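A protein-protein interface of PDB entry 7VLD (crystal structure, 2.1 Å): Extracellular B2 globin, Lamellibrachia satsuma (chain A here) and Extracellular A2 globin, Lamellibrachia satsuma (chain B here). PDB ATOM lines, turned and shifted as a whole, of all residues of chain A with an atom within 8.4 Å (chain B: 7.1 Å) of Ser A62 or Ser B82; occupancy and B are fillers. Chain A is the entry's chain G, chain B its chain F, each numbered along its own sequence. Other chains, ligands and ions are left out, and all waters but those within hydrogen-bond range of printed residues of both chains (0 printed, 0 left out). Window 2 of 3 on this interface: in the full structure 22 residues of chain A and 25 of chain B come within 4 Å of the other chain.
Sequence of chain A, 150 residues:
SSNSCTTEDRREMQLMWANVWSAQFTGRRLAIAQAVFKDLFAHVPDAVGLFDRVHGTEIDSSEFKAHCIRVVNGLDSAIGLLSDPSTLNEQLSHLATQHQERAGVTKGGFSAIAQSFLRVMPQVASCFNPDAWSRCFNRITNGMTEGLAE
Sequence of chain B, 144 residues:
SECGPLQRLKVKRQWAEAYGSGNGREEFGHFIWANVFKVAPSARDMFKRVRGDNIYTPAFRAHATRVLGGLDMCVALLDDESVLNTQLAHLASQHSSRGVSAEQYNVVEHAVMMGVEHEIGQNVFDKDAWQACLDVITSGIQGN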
ATOM      1  N   LEU A  30      12.560  -2.081  20.055  1.00  0.00           N
ATOM      2  CA  LEU A  30      13.727  -1.877  20.904  1.00  0.00           C
ATOM      3  C   LEU A  30      13.948  -3.059  21.839  1.00  0.00           C
ATOM      4  O   LEU A  30      15.086  -3.506  22.022  1.00  0.00           O
ATOM      5  CB  LEU A  30      13.552  -0.584  21.696  1.00  0.00           C
ATOM      6  CG  LEU A  30      14.771   0.145  22.242  1.00  0.00           C
ATOM      7  CD1 LEU A  30      15.816   0.337  21.158  1.00  0.00           C
ATOM      8  CD2 LEU A  30      14.300   1.478  22.773  1.00  0.00           C
ATOM      9  N   GLN A  34      17.349  -5.115  21.896  1.00  0.00           N
ATOM     10  CA  GLN A  34      18.159  -5.119  23.110  1.00  0.00           C
ATOM     11  C   GLN A  34      18.345  -6.534  23.643  1.00  0.00           C
ATOM     12  O   GLN A  34      19.425  -6.881  24.136  1.00  0.00           O
ATOM     13  CB  GLN A  34      17.525  -4.217  24.170  1.00  0.00           C
ATOM     14  CG  GLN A  34      17.599  -2.734  23.838  1.00  0.00           C
ATOM     15  CD  GLN A  34      16.888  -1.868  24.858  1.00  0.00           C
ATOM     16  OE1 GLN A  34      15.759  -2.156  25.256  1.00  0.00           O
ATOM     17  NE2 GLN A  34      17.550  -0.801  25.292  1.00  0.00           N
ATOM     18  N   VAL A  54      28.644   3.481  19.155  1.00  0.00           N
ATOM     19  CA  VAL A  54      27.230   3.527  19.501  1.00  0.00           C
ATOM     20  C   VAL A  54      27.001   3.143  20.963  1.00  0.00           C
ATOM     21  O   VAL A  54      25.878   2.834  21.350  1.00  0.00           O
ATOM     22  CB  VAL A  54      26.394   2.648  18.555  1.00  0.00           C
ATOM     23  CG1 VAL A  54      26.464   3.187  17.134  1.00  0.00           C
ATOM     24  CG2 VAL A  54      26.869   1.206  18.609  1.00  0.00           C
ATOM     25  N   HIS A  55      28.061   3.150  21.774  1.00  0.00           N
ATOM     26  CA  HIS A  55      27.958   2.969  23.225  1.00  0.00           C
ATOM     27  C   HIS A  55      27.406   1.588  23.582  1.00  0.00           C
ATOM     28  O   HIS A  55      26.441   1.455  24.338  1.00  0.00           O
ATOM     29  CB  HIS A  55      27.109   4.075  23.860  1.00  0.00           C
ATOM     30  CG  HIS A  55      27.646   5.457  23.646  1.00  0.00           C
ATOM     31  ND1 HIS A  55      27.440   6.479  24.546  1.00  0.00           N
ATOM     32  CD2 HIS A  55      28.372   5.988  22.634  1.00  0.00           C
ATOM     33  CE1 HIS A  55      28.020   7.579  24.101  1.00  0.00           C
ATOM     34  NE2 HIS A  55      28.592   7.309  22.942  1.00  0.00           N
ATOM     35  N   GLU A  58      26.660   0.602  27.242  1.00  0.00           N
ATOM     36  CA  GLU A  58      25.411   1.093  27.824  1.00  0.00           C
ATOM     37  C   GLU A  58      24.275   0.680  26.890  1.00  0.00           C
ATOM     38  O   GLU A  58      23.984   1.372  25.911  1.00  0.00           O
ATOM     39  CB  GLU A  58      25.440   2.607  28.019  1.00  0.00           C
ATOM     40  CG  GLU A  58      26.615   3.132  28.829  1.00  0.00           C
ATOM     41  CD  GLU A  58      27.802   3.510  27.963  1.00  0.00           C
ATOM     42  OE1 GLU A  58      27.832   3.106  26.783  1.00  0.00           O
ATOM     43  OE2 GLU A  58      28.703   4.216  28.463  1.00  0.00           O
ATOM     44  N   ILE A  59      23.631  -0.446  27.204  1.00  0.00           N
ATOM     45  CA  ILE A  59      22.587  -0.976  26.331  1.00  0.00           C
ATOM     46  C   ILE A  59      21.382  -0.042  26.286  1.00  0.00           C
ATOM     47  O   ILE A  59      20.664   0.009  25.279  1.00  0.00           O
ATOM     48  CB  ILE A  59      22.196  -2.396  26.786  1.00  0.00           C
ATOM     49  CG1 ILE A  59      23.437  -3.289  26.840  1.00  0.00           C
ATOM     50  CG2 ILE A  59      21.153  -3.001  25.857  1.00  0.00           C
ATOM     51  CD1 ILE A  59      23.192  -4.648  27.452  1.00  0.00           C
ATOM     52  N   ASP A  60      21.147   0.720  27.353  1.00  0.00           N
ATOM     53  CA  ASP A  60      19.988   1.597  27.450  1.00  0.00           C
ATOM     54  C   ASP A  60      20.295   3.046  27.087  1.00  0.00           C
ATOM     55  O   ASP A  60      19.439   3.913  27.287  1.00  0.00           O
ATOM     56  CB  ASP A  60      19.395   1.534  28.859  1.00  0.00           C
ATOM     57  CG  ASP A  60      18.206   0.601  28.949  1.00  0.00           C
ATOM     58  OD1 ASP A  60      17.622   0.277  27.894  1.00  0.00           O
ATOM     59  OD2 ASP A  60      17.850   0.199  30.076  1.00  0.00           O
ATOM     60  N   SER A  61      21.484   3.332  26.568  1.00  0.00           N
ATOM     61  CA  SER A  61      21.792   4.691  26.152  1.00  0.00           C
ATOM     62  C   SER A  61      21.034   5.043  24.875  1.00  0.00           C
ATOM     63  O   SER A  61      20.591   4.170  24.123  1.00  0.00           O
ATOM     64  CB  SER A  61      23.294   4.861  25.928  1.00  0.00           C
ATOM     65  OG  SER A  61      23.739   4.053  24.853  1.00  0.00           O
ATOM     66  N   SER A  62      20.886   6.348  24.636  1.00  0.00           N
ATOM     67  CA  SER A  62      20.239   6.801  23.408  1.00  0.00           C
ATOM     68  C   SER A  62      21.017   6.353  22.179  1.00  0.00           C
ATOM     69  O   SER A  62      20.424   5.962  21.166  1.00  0.00           O
ATOM     70  CB  SER A  62      20.089   8.322  23.419  1.00  0.00           C
ATOM     71  OG  SER A  62      19.132   8.738  24.376  1.00  0.00           O
ATOM     72  N   GLU A  63      22.349   6.394  22.254  1.00  0.00           N
ATOM     73  CA  GLU A  63      23.169   6.029  21.103  1.00  0.00           C
ATOM     74  C   GLU A  63      22.959   4.572  20.709  1.00  0.00           C
ATOM     75  O   GLU A  63      22.832   4.257  19.521  1.00  0.00           O
ATOM     76  CB  GLU A  63      24.644   6.300  21.401  1.00  0.00           C
ATOM     77  CG  GLU A  63      25.011   7.778  21.487  1.00  0.00           C
ATOM     78  CD  GLU A  63      24.802   8.367  22.871  1.00  0.00           C
ATOM     79  OE1 GLU A  63      24.203   7.689  23.733  1.00  0.00           O
ATOM     80  OE2 GLU A  63      25.247   9.513  23.099  1.00  0.00           O
ATOM     81  N   PHE A  64      22.912   3.668  21.690  1.00  0.00           N
ATOM     82  CA  PHE A  64      22.746   2.254  21.368  1.00  0.00           C
ATOM     83  C   PHE A  64      21.299   1.907  21.046  1.00  0.00           C
ATOM     84  O   PHE A  64      21.051   0.970  20.279  1.00  0.00           O
ATOM     85  CB  PHE A  64      23.258   1.380  22.513  1.00  0.00           C
ATOM     86  CG  PHE A  64      23.451  -0.059  22.130  1.00  0.00           C
ATOM     87  CD1 PHE A  64      24.487  -0.430  21.286  1.00  0.00           C
ATOM     88  CD2 PHE A  64      22.599  -1.040  22.606  1.00  0.00           C
ATOM     89  CE1 PHE A  64      24.669  -1.752  20.926  1.00  0.00           C
ATOM     90  CE2 PHE A  64      22.778  -2.366  22.250  1.00  0.00           C
ATOM     91  CZ  PHE A  64      23.814  -2.721  21.409  1.00  0.00           C
ATOM     92  N   LYS A  65      20.337   2.632  21.622  1.00  0.00           N
ATOM     93  CA  LYS A  65      18.947   2.470  21.207  1.00  0.00           C
ATOM     94  C   LYS A  65      18.772   2.821  19.738  1.00  0.00           C
ATOM     95  O   LYS A  65      18.088   2.107  18.997  1.00  0.00           O
ATOM     96  CB  LYS A  65      18.028   3.344  22.054  1.00  0.00           C
ATOM     97  CG  LYS A  65      17.801   2.881  23.469  1.00  0.00           C
ATOM     98  CD  LYS A  65      16.958   3.914  24.187  1.00  0.00           C
ATOM     99  CE  LYS A  65      16.775   3.579  25.643  1.00  0.00           C
ATOM    100  NZ  LYS A  65      15.629   4.331  26.213  1.00  0.00           N
ATOM    101  N   ALA A  66      19.365   3.937  19.306  1.00  0.00           N
ATOM    102  CA  ALA A  66      19.294   4.312  17.898  1.00  0.00           C
ATOM    103  C   ALA A  66      19.937   3.248  17.020  1.00  0.00           C
ATOM    104  O   ALA A  66      19.414   2.919  15.949  1.00  0.00           O
ATOM    105  CB  ALA A  66      19.960   5.670  17.682  1.00  0.00           C
ATOM    106  N   HIS A  67      21.067   2.690  17.463  1.00  0.00           N
ATOM    107  CA  HIS A  67      21.695   1.607  16.713  1.00  0.00           C
ATOM    108  C   HIS A  67      20.801   0.373  16.675  1.00  0.00           C
ATOM    109  O   HIS A  67      20.679  -0.280  15.631  1.00  0.00           O
ATOM    110  CB  HIS A  67      23.055   1.259  17.317  1.00  0.00           C
ATOM    111  CG  HIS A  67      23.662   0.017  16.745  1.00  0.00           C
ATOM    112  ND1 HIS A  67      24.198  -0.032  15.476  1.00  0.00           N
ATOM    113  CD2 HIS A  67      23.802  -1.227  17.261  1.00  0.00           C
ATOM    114  CE1 HIS A  67      24.651  -1.250  15.239  1.00  0.00           C
ATOM    115  NE2 HIS A  67      24.422  -1.995  16.306  1.00  0.00           N
ATOM    116  N   CYS A  68      20.175   0.034  17.805  1.00  0.00           N
ATOM    117  CA  CYS A  68      19.260  -1.103  17.836  1.00  0.00           C
ATOM    118  C   CYS A  68      18.116  -0.920  16.847  1.00  0.00           C
ATOM    119  O   CYS A  68      17.726  -1.865  16.151  1.00  0.00           O
ATOM    120  CB  CYS A  68      18.709  -1.296  19.251  1.00  0.00           C
ATOM    121  SG  CYS A  68      19.840  -2.103  20.402  1.00  0.00           S
ATOM    122  N   ILE A  69      17.566   0.292  16.774  1.00  0.00           N
ATOM    123  CA  ILE A  69      16.458   0.560  15.865  1.00  0.00           C
ATOM    124  C   ILE A  69      16.919   0.464  14.415  1.00  0.00           C
ATOM    125  O   ILE A  69      16.185  -0.024  13.547  1.00  0.00           O
ATOM    126  CB  ILE A  69      15.839   1.931  16.194  1.00  0.00           C
ATOM    127  CG1 ILE A  69      15.087   1.845  17.523  1.00  0.00           C
ATOM    128  CG2 ILE A  69      14.926   2.407  15.074  1.00  0.00           C
ATOM    129  CD1 ILE A  69      14.701   3.177  18.094  1.00  0.00           C
ATOM    130  N   ARG A  70      18.146   0.906  14.130  1.00  0.00           N
ATOM    131  CA  ARG A  70      18.676   0.777  12.776  1.00  0.00           C
ATOM    132  C   ARG A  70      18.881  -0.684  12.397  1.00  0.00           C
ATOM    133  O   ARG A  70      18.642  -1.071  11.248  1.00  0.00           O
ATOM    134  CB  ARG A  70      19.987   1.556  12.642  1.00  0.00           C
ATOM    135  CG  ARG A  70      19.820   3.068  12.688  1.00  0.00           C
ATOM    136  CD  ARG A  70      21.090   3.796  12.264  1.00  0.00           C
ATOM    137  NE  ARG A  70      22.170   3.660  13.241  1.00  0.00           N
ATOM    138  CZ  ARG A  70      22.364   4.493  14.259  1.00  0.00           C
ATOM    139  NH1 ARG A  70      21.547   5.521  14.443  1.00  0.00           N
ATOM    140  NH2 ARG A  70      23.373   4.295  15.095  1.00  0.00           N
ATOM    141  N   LEU B  77       9.851   7.086  16.142  1.00  0.00           N
ATOM    142  CA  LEU B  77      10.558   7.715  17.250  1.00  0.00           C
ATOM    143  C   LEU B  77      10.032   9.101  17.597  1.00  0.00           C
ATOM    144  O   LEU B  77      10.601   9.757  18.475  1.00  0.00           O
ATOM    145  CB  LEU B  77      12.055   7.803  16.935  1.00  0.00           C
ATOM    146  CG  LEU B  77      12.849   6.514  17.145  1.00  0.00           C
ATOM    147  CD1 LEU B  77      14.277   6.668  16.648  1.00  0.00           C
ATOM    148  CD2 LEU B  77      12.825   6.140  18.615  1.00  0.00           C
ATOM    149  N   ASP B  79       7.695  10.039  19.358  1.00  0.00           N
ATOM    150  CA  ASP B  79       7.315  10.119  20.762  1.00  0.00           C
ATOM    151  C   ASP B  79       8.504  10.004  21.708  1.00  0.00           C
ATOM    152  O   ASP B  79       8.316  10.086  22.926  1.00  0.00           O
ATOM    153  CB  ASP B  79       6.300   9.022  21.097  1.00  0.00           C
ATOM    154  CG  ASP B  79       6.875   7.630  20.925  1.00  0.00           C
ATOM    155  OD1 ASP B  79       7.250   7.273  19.789  1.00  0.00           O
ATOM    156  OD2 ASP B  79       6.972   6.897  21.932  1.00  0.00           O
ATOM    157  N   ASP B  80       9.715   9.810  21.182  1.00  0.00           N
ATOM    158  CA  ASP B  80      10.926   9.610  21.984  1.00  0.00           C
ATOM    159  C   ASP B  80      11.952  10.641  21.513  1.00  0.00           C
ATOM    160  O   ASP B  80      12.812  10.338  20.683  1.00  0.00           O
ATOM    161  CB  ASP B  80      11.437   8.173  21.841  1.00  0.00           C
ATOM    162  CG  ASP B  80      12.463   7.804  22.896  1.00  0.00           C
ATOM    163  OD1 ASP B  80      13.120   8.712  23.446  1.00  0.00           O
ATOM    164  OD2 ASP B  80      12.615   6.595  23.172  1.00  0.00           O
ATOM    165  N   GLU B  81      11.862  11.856  22.064  1.00  0.00           N
ATOM    166  CA  GLU B  81      12.644  12.977  21.549  1.00  0.00           C
ATOM    167  C   GLU B  81      14.144  12.714  21.647  1.00  0.00           C
ATOM    168  O   GLU B  81      14.904  13.085  20.744  1.00  0.00           O
ATOM    169  CB  GLU B  81      12.277  14.258  22.300  1.00  0.00           C
ATOM    170  CG  GLU B  81      13.057  15.487  21.856  1.00  0.00           C
ATOM    171  CD  GLU B  81      12.213  16.464  21.061  1.00  0.00           C
ATOM    172  OE1 GLU B  81      12.486  17.681  21.135  1.00  0.00           O
ATOM    173  OE2 GLU B  81      11.275  16.019  20.366  1.00  0.00           O
ATOM    174  N   SER B  82      14.587  12.077  22.733  1.00  0.00           N
ATOM    175  CA  SER B  82      16.014  11.821  22.911  1.00  0.00           C
ATOM    176  C   SER B  82      16.547  10.889  21.828  1.00  0.00           C
ATOM    177  O   SER B  82      17.546  11.193  21.166  1.00  0.00           O
ATOM    178  CB  SER B  82      16.271  11.234  24.299  1.00  0.00           C
ATOM    179  OG  SER B  82      17.634  10.875  24.450  1.00  0.00           O
ATOM    180  N   VAL B  83      15.889   9.744  21.635  1.00  0.00           N
ATOM    181  CA  VAL B  83      16.346   8.794  20.627  1.00  0.00           C
ATOM    182  C   VAL B  83      16.040   9.307  19.223  1.00  0.00           C
ATOM    183  O   VAL B  83      16.775   9.008  18.272  1.00  0.00           O
ATOM    184  CB  VAL B  83      15.720   7.411  20.883  1.00  0.00           C
ATOM    185  CG1 VAL B  83      16.285   6.374  19.922  1.00  0.00           C
ATOM    186  CG2 VAL B  83      15.953   6.988  22.330  1.00  0.00           C
ATOM    187  N   LEU B  84      14.968  10.088  19.067  1.00  0.00           N
ATOM    188  CA  LEU B  84      14.661  10.677  17.766  1.00  0.00           C
ATOM    189  C   LEU B  84      15.792  11.582  17.294  1.00  0.00           C
ATOM    190  O   LEU B  84      16.232  11.497  16.142  1.00  0.00           O
ATOM    191  CB  LEU B  84      13.347  11.457  17.835  1.00  0.00           C
ATOM    192  CG  LEU B  84      13.034  12.343  16.626  1.00  0.00           C
ATOM    193  CD1 LEU B  84      12.769  11.502  15.384  1.00  0.00           C
ATOM    194  CD2 LEU B  84      11.862  13.270  16.918  1.00  0.00           C
ATOM    195  N   ASN B  85      16.277  12.459  18.177  1.00  0.00           N
ATOM    196  CA  ASN B  85      17.329  13.391  17.788  1.00  0.00           C
ATOM    197  C   ASN B  85      18.650  12.677  17.530  1.00  0.00           C
ATOM    198  O   ASN B  85      19.458  13.147  16.721  1.00  0.00           O
ATOM    199  CB  ASN B  85      17.497  14.469  18.859  1.00  0.00           C
ATOM    200  CG  ASN B  85      16.324  15.430  18.900  1.00  0.00           C
ATOM    201  OD1 ASN B  85      15.692  15.696  17.877  1.00  0.00           O
ATOM    202  ND2 ASN B  85      16.028  15.957  20.082  1.00  0.00           N
ATOM    203  N   THR B  86      18.887  11.548  18.201  1.00  0.00           N
ATOM    204  CA  THR B  86      20.073  10.754  17.900  1.00  0.00           C
ATOM    205  C   THR B  86      19.992  10.161  16.498  1.00  0.00           C
ATOM    206  O   THR B  86      20.970  10.202  15.742  1.00  0.00           O
ATOM    207  CB  THR B  86      20.244   9.646  18.939  1.00  0.00           C
ATOM    208  OG1 THR B  86      20.202  10.214  20.254  1.00  0.00           O
ATOM    209  CG2 THR B  86      21.577   8.935  18.745  1.00  0.00           C
ATOM    210  N   GLN B  87      18.830   9.613  16.132  1.00  0.00           N
ATOM    211  CA  GLN B  87      18.662   9.076  14.786  1.00  0.00           C
ATOM    212  C   GLN B  87      18.696  10.184  13.742  1.00  0.00           C
ATOM    213  O   GLN B  87      19.258  10.003  12.655  1.00  0.00           O
ATOM    214  CB  GLN B  87      17.356   8.286  14.695  1.00  0.00           C
ATOM    215  CG  GLN B  87      17.050   7.751  13.304  1.00  0.00           C
ATOM    216  CD  GLN B  87      18.149   6.856  12.765  1.00  0.00           C
ATOM    217  OE1 GLN B  87      18.792   6.122  13.514  1.00  0.00           O
ATOM    218  NE2 GLN B  87      18.371   6.917  11.457  1.00  0.00           N
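Printed residues of chain A that touch a printed residue of chain B: Ser A62, Lys A65, Ala A66, Ile A69 and Arg A70.
Hydrophobic or aromatic side chains of chain B within 4 Å of the printed part of chain A: Leu B77 and Val B83.
Among the printed residues, 7 pairs touch across the chains.
Among the printed residues, no Asp or Glu carboxylate lies within 4 Å of a Lys or Arg side-chain nitrogen of the other chain.
His A55 touches none of the printed residues of chain B.
Ser A62 touches just these residues of chain B: Ser B82 and Thr B86.
Printed residues of chain B within 4 Å of Lys A65: Val B83 (3.7 Å).
Printed residues of chain A within 4 Å of Leu B77: Ile A69 (3.5 Å).
Of chain A, only Ser A62 (2.6 Å) comes within 4 Å of Ser B82.
Of the printed residues of chain A, Gln B87 touches Arg A70.
The nearest residue of chain B that does not touch Ser A62 is Val B83 (4.2 Å).
The nearest residue of chain A that does not touch Ser B82 is Ser A61 (6.8 Å).
The nearest printed residue of chain A that does not touch Gln B87 is Ala A66 (4.1 Å).
OD1 of Asp B80 sits at hydrogen-bond distance from N of Val B83.
The backbone carbonyl oxygen of Ser B82 is in hydrogen-bond range of the side-chain hydroxyl of Thr B86, at 3.0 Å.
Ser A62 touches Thr B86.
Lys A65 touches Val B83.
Ala A66 touches Val B83.
Ala A66 touches Thr B86 (CB to CG2, 3.8 Å).
Ile A69 touches Leu B77 (CD1 to CD2, 3.5 Å).
OG of Ser A62 sits at hydrogen-bond distance from OG of Ser B82 (2.6 Å).
OE1 of Gln B87 sits at hydrogen-bond distance from NH1 of Arg A70 (3.0 Å).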
